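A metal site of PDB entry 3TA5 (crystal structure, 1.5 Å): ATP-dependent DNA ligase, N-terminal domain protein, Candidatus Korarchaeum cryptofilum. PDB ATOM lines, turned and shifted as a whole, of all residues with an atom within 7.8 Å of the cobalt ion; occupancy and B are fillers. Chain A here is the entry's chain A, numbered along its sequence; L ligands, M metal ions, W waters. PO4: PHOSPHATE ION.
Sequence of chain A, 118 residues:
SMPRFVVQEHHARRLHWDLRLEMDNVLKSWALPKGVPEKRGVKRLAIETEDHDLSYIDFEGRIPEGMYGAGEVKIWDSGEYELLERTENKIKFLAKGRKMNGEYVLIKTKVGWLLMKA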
ATOM      1  N   GLN A   8      -7.979  19.478 -20.219  1.00  0.00           N
ATOM      2  CA  GLN A   8      -6.597  19.023 -20.378  1.00  0.00           C
ATOM      3  C   GLN A   8      -5.908  19.206 -19.045  1.00  0.00           C
ATOM      4  O   GLN A   8      -6.093  20.207 -18.371  1.00  0.00           O
ATOM      5  CB  GLN A   8      -5.873  19.872 -21.420  1.00  0.00           C
ATOM      6  CG  GLN A   8      -6.366  19.656 -22.829  1.00  0.00           C
ATOM      7  CD  GLN A   8      -5.988  20.813 -23.736  1.00  0.00           C
ATOM      8  OE1 GLN A   8      -5.607  21.891 -23.277  1.00  0.00           O
ATOM      9  NE2 GLN A   8      -6.011  20.560 -25.051  1.00  0.00           N
ATOM     10  N   GLU A   9      -5.097  18.229 -18.669  1.00  0.00           N
ATOM     11  CA  GLU A   9      -4.241  18.385 -17.502  1.00  0.00           C
ATOM     12  C   GLU A   9      -2.876  18.833 -18.019  1.00  0.00           C
ATOM     13  O   GLU A   9      -2.273  18.198 -18.883  1.00  0.00           O
ATOM     14  CB  GLU A   9      -4.165  17.088 -16.703  1.00  0.00           C
ATOM     15  CG  GLU A   9      -3.296  17.178 -15.437  1.00  0.00           C
ATOM     16  CD  GLU A   9      -3.402  15.979 -14.508  1.00  0.00           C
ATOM     17  OE1 GLU A   9      -4.487  15.417 -14.340  1.00  0.00           O
ATOM     18  OE2 GLU A   9      -2.368  15.610 -13.907  1.00  0.00           O
ATOM     19  N   HIS A  10      -2.407  19.954 -17.473  1.00  0.00           N
ATOM     20  CA  HIS A  10      -1.259  20.678 -18.004  1.00  0.00           C
ATOM     21  C   HIS A  10      -0.175  20.775 -16.930  1.00  0.00           C
ATOM     22  O   HIS A  10      -0.299  21.555 -15.988  1.00  0.00           O
ATOM     23  CB  HIS A  10      -1.731  22.068 -18.402  1.00  0.00           C
ATOM     24  CG  HIS A  10      -0.783  22.803 -19.292  1.00  0.00           C
ATOM     25  ND1 HIS A  10      -1.102  24.012 -19.868  1.00  0.00           N
ATOM     26  CD2 HIS A  10       0.463  22.495 -19.711  1.00  0.00           C
ATOM     27  CE1 HIS A  10      -0.079  24.429 -20.592  1.00  0.00           C
ATOM     28  NE2 HIS A  10       0.882  23.524 -20.531  1.00  0.00           N
ATOM     29  N   HIS A  11       0.872  19.977 -17.085  1.00  0.00           N
ATOM     30  CA  HIS A  11       2.015  19.980 -16.172  1.00  0.00           C
ATOM     31  C   HIS A  11       3.022  21.056 -16.561  1.00  0.00           C
ATOM     32  O   HIS A  11       4.037  20.769 -17.190  1.00  0.00           O
ATOM     33  CB  HIS A  11       2.656  18.599 -16.129  1.00  0.00           C
ATOM     34  CG  HIS A  11       1.787  17.560 -15.478  1.00  0.00           C
ATOM     35  ND1 HIS A  11       2.225  16.295 -15.162  1.00  0.00           N
ATOM     36  CD2 HIS A  11       0.496  17.639 -15.053  1.00  0.00           C
ATOM     37  CE1 HIS A  11       1.234  15.626 -14.593  1.00  0.00           C
ATOM     38  NE2 HIS A  11       0.182  16.414 -14.516  1.00  0.00           N
ATOM     39  N   ALA A  12       2.708  22.284 -16.165  1.00  0.00           N
ATOM     40  CA  ALA A  12       3.521  23.462 -16.396  1.00  0.00           C
ATOM     41  C   ALA A  12       4.133  23.909 -15.060  1.00  0.00           C
ATOM     42  O   ALA A  12       4.026  23.221 -14.046  1.00  0.00           O
ATOM     43  CB  ALA A  12       2.655  24.565 -16.963  1.00  0.00           C
ATOM     44  N   ARG A  14       3.107  25.996 -13.007  1.00  0.00           N
ATOM     45  CA  ARG A  14       2.010  25.814 -12.066  1.00  0.00           C
ATOM     46  C   ARG A  14       1.073  24.782 -12.668  1.00  0.00           C
ATOM     47  O   ARG A  14       0.473  25.031 -13.705  1.00  0.00           O
ATOM     48  CB  ARG A  14       1.271  27.124 -11.772  1.00  0.00           C
ATOM     49  CG  ARG A  14       2.086  28.137 -10.947  1.00  0.00           C
ATOM     50  CD  ARG A  14       1.264  29.388 -10.637  1.00  0.00           C
ATOM     51  NE  ARG A  14       2.052  30.438  -9.970  1.00  0.00           N
ATOM     52  CZ  ARG A  14       1.548  31.612  -9.572  1.00  0.00           C
ATOM     53  NH1 ARG A  14       0.269  31.906  -9.777  1.00  0.00           N
ATOM     54  NH2 ARG A  14       2.340  32.507  -8.983  1.00  0.00           N
ATOM     55  N   LEU A  15       0.995  23.609 -12.048  1.00  0.00           N
ATOM     56  CA  LEU A  15       0.125  22.535 -12.529  1.00  0.00           C
ATOM     57  C   LEU A  15      -1.326  23.008 -12.467  1.00  0.00           C
ATOM     58  O   LEU A  15      -1.771  23.609 -11.499  1.00  0.00           O
ATOM     59  CB  LEU A  15       0.357  21.241 -11.730  1.00  0.00           C
ATOM     60  CG  LEU A  15      -0.416  19.953 -12.059  1.00  0.00           C
ATOM     61  CD1 LEU A  15       0.094  18.778 -11.253  1.00  0.00           C
ATOM     62  CD2 LEU A  15      -1.881  20.127 -11.784  1.00  0.00           C
ATOM     63  N   HIS A  16      -2.082  22.733 -13.523  1.00  0.00           N
ATOM     64  CA  HIS A  16      -3.469  23.174 -13.583  1.00  0.00           C
ATOM     65  C   HIS A  16      -4.196  22.338 -14.642  1.00  0.00           C
ATOM     66  O   HIS A  16      -3.583  21.528 -15.362  1.00  0.00           O
ATOM     67  CB  HIS A  16      -3.537  24.676 -13.953  1.00  0.00           C
ATOM     68  CG  HIS A  16      -2.951  24.972 -15.298  1.00  0.00           C
ATOM     69  ND1 HIS A  16      -1.597  25.051 -15.517  1.00  0.00           N
ATOM     70  CD2 HIS A  16      -3.548  25.182 -16.493  1.00  0.00           C
ATOM     71  CE1 HIS A  16      -1.369  25.276 -16.800  1.00  0.00           C
ATOM     72  NE2 HIS A  16      -2.537  25.364 -17.416  1.00  0.00           N
ATOM     73  N   TRP A  17      -5.491  22.572 -14.760  1.00  0.00           N
ATOM     74  CA  TRP A  17      -6.338  21.931 -15.716  1.00  0.00           C
ATOM     75  C   TRP A  17      -7.020  22.979 -16.571  1.00  0.00           C
ATOM     76  O   TRP A  17      -7.554  23.957 -16.054  1.00  0.00           O
ATOM     77  CB  TRP A  17      -7.403  21.067 -15.015  1.00  0.00           C
ATOM     78  CG  TRP A  17      -6.860  19.872 -14.379  1.00  0.00           C
ATOM     79  CD1 TRP A  17      -6.855  18.603 -14.881  1.00  0.00           C
ATOM     80  CD2 TRP A  17      -6.200  19.802 -13.106  1.00  0.00           C
ATOM     81  NE1 TRP A  17      -6.253  17.736 -13.993  1.00  0.00           N
ATOM     82  CE2 TRP A  17      -5.816  18.456 -12.914  1.00  0.00           C
ATOM     83  CE3 TRP A  17      -5.874  20.750 -12.133  1.00  0.00           C
ATOM     84  CZ2 TRP A  17      -5.132  18.041 -11.769  1.00  0.00           C
ATOM     85  CZ3 TRP A  17      -5.204  20.318 -10.980  1.00  0.00           C
ATOM     86  CH2 TRP A  17      -4.836  18.975 -10.829  1.00  0.00           C
ATOM     87  N   ASP A  18      -7.014  22.778 -17.878  1.00  0.00           N
ATOM     88  CA  ASP A  18      -7.626  23.744 -18.770  1.00  0.00           C
ATOM     89  C   ASP A  18      -8.952  23.191 -19.296  1.00  0.00           C
ATOM     90  O   ASP A  18      -8.973  22.130 -19.941  1.00  0.00           O
ATOM     91  CB  ASP A  18      -6.694  24.041 -19.957  1.00  0.00           C
ATOM     92  CG  ASP A  18      -5.481  24.849 -19.552  1.00  0.00           C
ATOM     93  OD1 ASP A  18      -5.651  25.936 -18.980  1.00  0.00           O
ATOM     94  OD2 ASP A  18      -4.361  24.373 -19.831  1.00  0.00           O
ATOM     95  N   LEU A  19     -10.030  23.897 -19.013  1.00  0.00           N
ATOM     96  CA  LEU A  19     -11.347  23.572 -19.549  1.00  0.00           C
ATOM     97  C   LEU A  19     -11.555  24.348 -20.827  1.00  0.00           C
ATOM     98  O   LEU A  19     -11.395  25.567 -20.828  1.00  0.00           O
ATOM     99  CB  LEU A  19     -12.406  23.947 -18.512  1.00  0.00           C
ATOM    100  CG  LEU A  19     -13.840  23.896 -19.029  1.00  0.00           C
ATOM    101  CD1 LEU A  19     -14.269  22.475 -19.317  1.00  0.00           C
ATOM    102  CD2 LEU A  19     -14.755  24.546 -17.983  1.00  0.00           C
ATOM    103  N   ARG A  20     -11.869  23.639 -21.909  1.00  0.00           N
ATOM    104  CA  ARG A  20     -12.068  24.295 -23.202  1.00  0.00           C
ATOM    105  C   ARG A  20     -13.397  23.849 -23.817  1.00  0.00           C
ATOM    106  O   ARG A  20     -13.646  22.649 -23.922  1.00  0.00           O
ATOM    107  CB  ARG A  20     -10.903  23.989 -24.158  1.00  0.00           C
ATOM    108  CG  ARG A  20      -9.508  24.258 -23.540  1.00  0.00           C
ATOM    109  CD  ARG A  20      -8.436  24.243 -24.633  1.00  0.00           C
ATOM    110  NE  ARG A  20      -7.088  24.162 -24.060  1.00  0.00           N
ATOM    111  CZ  ARG A  20      -6.425  25.212 -23.556  1.00  0.00           C
ATOM    112  NH1 ARG A  20      -6.959  26.428 -23.612  1.00  0.00           N
ATOM    113  NH2 ARG A  20      -5.199  25.057 -23.038  1.00  0.00           N
ATOM    114  N   TRP A  30     -10.620  28.256 -19.975  1.00  0.00           N
ATOM    115  CA  TRP A  30     -10.397  28.663 -18.581  1.00  0.00           C
ATOM    116  C   TRP A  30      -9.367  27.714 -17.962  1.00  0.00           C
ATOM    117  O   TRP A  30      -9.500  26.495 -18.069  1.00  0.00           O
ATOM    118  CB  TRP A  30     -11.668  28.561 -17.757  1.00  0.00           C
ATOM    119  CG  TRP A  30     -12.725  29.568 -18.089  1.00  0.00           C
ATOM    120  CD1 TRP A  30     -12.976  30.739 -17.451  1.00  0.00           C
ATOM    121  CD2 TRP A  30     -13.690  29.471 -19.144  1.00  0.00           C
ATOM    122  NE1 TRP A  30     -14.030  31.385 -18.047  1.00  0.00           N
ATOM    123  CE2 TRP A  30     -14.492  30.616 -19.088  1.00  0.00           C
ATOM    124  CE3 TRP A  30     -13.953  28.501 -20.143  1.00  0.00           C
ATOM    125  CZ2 TRP A  30     -15.538  30.858 -19.986  1.00  0.00           C
ATOM    126  CZ3 TRP A  30     -14.999  28.743 -21.041  1.00  0.00           C
ATOM    127  CH2 TRP A  30     -15.782  29.908 -20.946  1.00  0.00           C
ATOM    128  N   ALA A  31      -8.378  28.288 -17.276  1.00  0.00           N
ATOM    129  CA  ALA A  31      -7.452  27.488 -16.466  1.00  0.00           C
ATOM    130  C   ALA A  31      -8.016  27.289 -15.067  1.00  0.00           C
ATOM    131  O   ALA A  31      -8.595  28.203 -14.486  1.00  0.00           O
ATOM    132  CB  ALA A  31      -6.071  28.165 -16.411  1.00  0.00           C
ATOM    133  N   LEU A  32      -7.937  26.065 -14.570  1.00  0.00           N
ATOM    134  CA  LEU A  32      -8.497  25.704 -13.283  1.00  0.00           C
ATOM    135  C   LEU A  32      -7.343  25.217 -12.399  1.00  0.00           C
ATOM    136  O   LEU A  32      -6.886  24.071 -12.537  1.00  0.00           O
ATOM    137  CB  LEU A  32      -9.524  24.576 -13.465  1.00  0.00           C
ATOM    138  CG  LEU A  32     -10.661  24.735 -14.491  1.00  0.00           C
ATOM    139  CD1 LEU A  32     -11.453  23.428 -14.597  1.00  0.00           C
ATOM    140  CD2 LEU A  32     -11.536  25.892 -14.117  1.00  0.00           C
ATOM    141  N   THR A  49      -8.795  32.443 -20.065  1.00  0.00           N
ATOM    142  CA  THR A  49      -7.570  32.530 -20.842  1.00  0.00           C
ATOM    143  C   THR A  49      -7.918  32.764 -22.327  1.00  0.00           C
ATOM    144  O   THR A  49      -9.084  32.884 -22.673  1.00  0.00           O
ATOM    145  CB  THR A  49      -6.711  31.261 -20.653  1.00  0.00           C
ATOM    146  OG1 THR A  49      -7.436  30.115 -21.130  1.00  0.00           O
ATOM    147  CG2 THR A  49      -6.362  31.040 -19.180  1.00  0.00           C
ATOM    148  N   HIS A  52      -8.504  29.315 -28.062  1.00  0.00           N
ATOM    149  CA  HIS A  52      -7.638  28.408 -28.795  1.00  0.00           C
ATOM    150  C   HIS A  52      -8.374  27.938 -30.039  1.00  0.00           C
ATOM    151  O   HIS A  52      -9.585  28.063 -30.132  1.00  0.00           O
ATOM    152  CB  HIS A  52      -7.203  27.212 -27.942  1.00  0.00           C
ATOM    153  CG  HIS A  52      -6.123  27.542 -26.951  1.00  0.00           C
ATOM    154  ND1 HIS A  52      -6.236  28.575 -26.043  1.00  0.00           N
ATOM    155  CD2 HIS A  52      -4.914  26.985 -26.735  1.00  0.00           C
ATOM    156  CE1 HIS A  52      -5.140  28.629 -25.309  1.00  0.00           C
ATOM    157  NE2 HIS A  52      -4.329  27.674 -25.710  1.00  0.00           N
ATOM    158  N   TYR A  56      -7.212  22.176 -31.618  1.00  0.00           N
ATOM    159  CA  TYR A  56      -6.435  21.873 -30.412  1.00  0.00           C
ATOM    160  C   TYR A  56      -7.192  20.982 -29.435  1.00  0.00           C
ATOM    161  O   TYR A  56      -6.615  20.498 -28.447  1.00  0.00           O
ATOM    162  CB  TYR A  56      -6.042  23.181 -29.734  1.00  0.00           C
ATOM    163  CG  TYR A  56      -4.940  23.075 -28.696  1.00  0.00           C
ATOM    164  CD1 TYR A  56      -3.630  22.750 -29.086  1.00  0.00           C
ATOM    165  CD2 TYR A  56      -5.173  23.354 -27.351  1.00  0.00           C
ATOM    166  CE1 TYR A  56      -2.606  22.667 -28.149  1.00  0.00           C
ATOM    167  CE2 TYR A  56      -4.126  23.292 -26.407  1.00  0.00           C
ATOM    168  CZ  TYR A  56      -2.869  22.930 -26.815  1.00  0.00           C
ATOM    169  OH  TYR A  56      -1.826  22.871 -25.883  1.00  0.00           O
ATOM    170  N   TYR A  68       5.038  30.134 -24.462  1.00  0.00           N
ATOM    171  CA  TYR A  68       3.999  30.435 -23.485  1.00  0.00           C
ATOM    172  C   TYR A  68       3.052  29.250 -23.408  1.00  0.00           C
ATOM    173  O   TYR A  68       2.298  28.984 -24.355  1.00  0.00           O
ATOM    174  CB  TYR A  68       3.245  31.704 -23.859  1.00  0.00           C
ATOM    175  CG  TYR A  68       2.270  32.141 -22.782  1.00  0.00           C
ATOM    176  CD1 TYR A  68       2.713  32.425 -21.499  1.00  0.00           C
ATOM    177  CD2 TYR A  68       0.915  32.244 -23.053  1.00  0.00           C
ATOM    178  CE1 TYR A  68       1.848  32.823 -20.513  1.00  0.00           C
ATOM    179  CE2 TYR A  68       0.037  32.639 -22.072  1.00  0.00           C
ATOM    180  CZ  TYR A  68       0.505  32.923 -20.812  1.00  0.00           C
ATOM    181  OH  TYR A  68      -0.366  33.312 -19.827  1.00  0.00           O
ATOM    182  N   GLY A  69       3.106  28.547 -22.269  1.00  0.00           N
ATOM    183  CA  GLY A  69       2.320  27.354 -22.035  1.00  0.00           C
ATOM    184  C   GLY A  69       3.147  26.074 -21.978  1.00  0.00           C
ATOM    185  O   GLY A  69       2.608  24.981 -22.164  1.00  0.00           O
ATOM    186  N   ALA A  70       4.450  26.203 -21.744  1.00  0.00           N
ATOM    187  CA  ALA A  70       5.342  25.044 -21.739  1.00  0.00           C
ATOM    188  C   ALA A  70       4.835  23.946 -20.806  1.00  0.00           C
ATOM    189  O   ALA A  70       4.194  24.235 -19.790  1.00  0.00           O
ATOM    190  CB  ALA A  70       6.755  25.458 -21.336  1.00  0.00           C
ATOM    191  N   GLU A  72       3.765  19.399 -20.290  1.00  0.00           N
ATOM    192  CA  GLU A  72       3.042  18.278 -20.867  1.00  0.00           C
ATOM    193  C   GLU A  72       1.535  18.466 -20.776  1.00  0.00           C
ATOM    194  O   GLU A  72       1.015  18.819 -19.714  1.00  0.00           O
ATOM    195  CB  GLU A  72       3.413  16.985 -20.141  1.00  0.00           C
ATOM    196  CG  GLU A  72       2.978  15.727 -20.853  1.00  0.00           C
ATOM    197  CD  GLU A  72       4.115  15.089 -21.632  1.00  0.00           C
ATOM    198  OE1 GLU A  72       4.969  14.414 -21.008  1.00  0.00           O
ATOM    199  OE2 GLU A  72       4.162  15.272 -22.866  1.00  0.00           O
ATOM    200  N   VAL A  73       0.861  18.246 -21.902  1.00  0.00           N
ATOM    201  CA  VAL A  73      -0.596  18.320 -21.951  1.00  0.00           C
ATOM    202  C   VAL A  73      -1.160  16.934 -22.180  1.00  0.00           C
ATOM    203  O   VAL A  73      -0.765  16.241 -23.115  1.00  0.00           O
ATOM    204  CB  VAL A  73      -1.040  19.238 -23.116  1.00  0.00           C
ATOM    205  CG1 VAL A  73      -2.558  19.296 -23.222  1.00  0.00           C
ATOM    206  CG2 VAL A  73      -0.467  20.651 -22.951  1.00  0.00           C
HETATM  207  P   PO4 L   1      -2.465  27.456 -22.128  1.00  0.00           P
HETATM  208  O1  PO4 L   1      -2.478  27.247 -23.640  1.00  0.00           O
HETATM  209  O2  PO4 L   1      -1.088  27.978 -21.774  1.00  0.00           O
HETATM  210  O3  PO4 L   1      -3.564  28.480 -21.890  1.00  0.00           O
HETATM  211  O4  PO4 L   1      -2.857  26.139 -21.527  1.00  0.00           O
HETATM  212 CO    CO M   1      -2.690  25.490 -19.538  1.00  0.00          CO
HETATM  213  O   HOH W   1      -3.844  27.578 -19.036  1.00  0.00           O
HETATM  214  O   HOH W   2      -0.864  27.121 -19.596  1.00  0.00           O
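OD2 of Asp 18 sits close to NH2 of Arg 20, at 3.4 Å. The backbone carbonyl oxygen (O) of Gln 8 is in hydrogen-bond range of the backbone NH (N) of Asp 18, at 2.8 Å. A ring nitrogen (ND1) of His 16 is in hydrogen-bond range of the backbone carbonyl oxygen of Arg 14 (2.8 Å). A ring nitrogen (NE2) of His 10 is in hydrogen-bond range of the backbone carbonyl oxygen of Gly 69 (2.8 Å). A ring nitrogen (NE2) of His 10 is in hydrogen-bond range of the backbone carbonyl oxygen (O) of Ala 70 (3.5 Å).
Of the 23 residues printed, 3 come within 4 Å of the cobalt ion.
The cobalt ion is bound by OD2 of Asp 18 (2.0 Å), O4 of the ligand (2.1 Å), NE2 of His 16 (2.1 Å), ND1 of His 10 (2.2 Å), water W1 (2.4 Å) and water W2 (2.4 Å). The cobalt ion has six donor atoms within binding distance.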
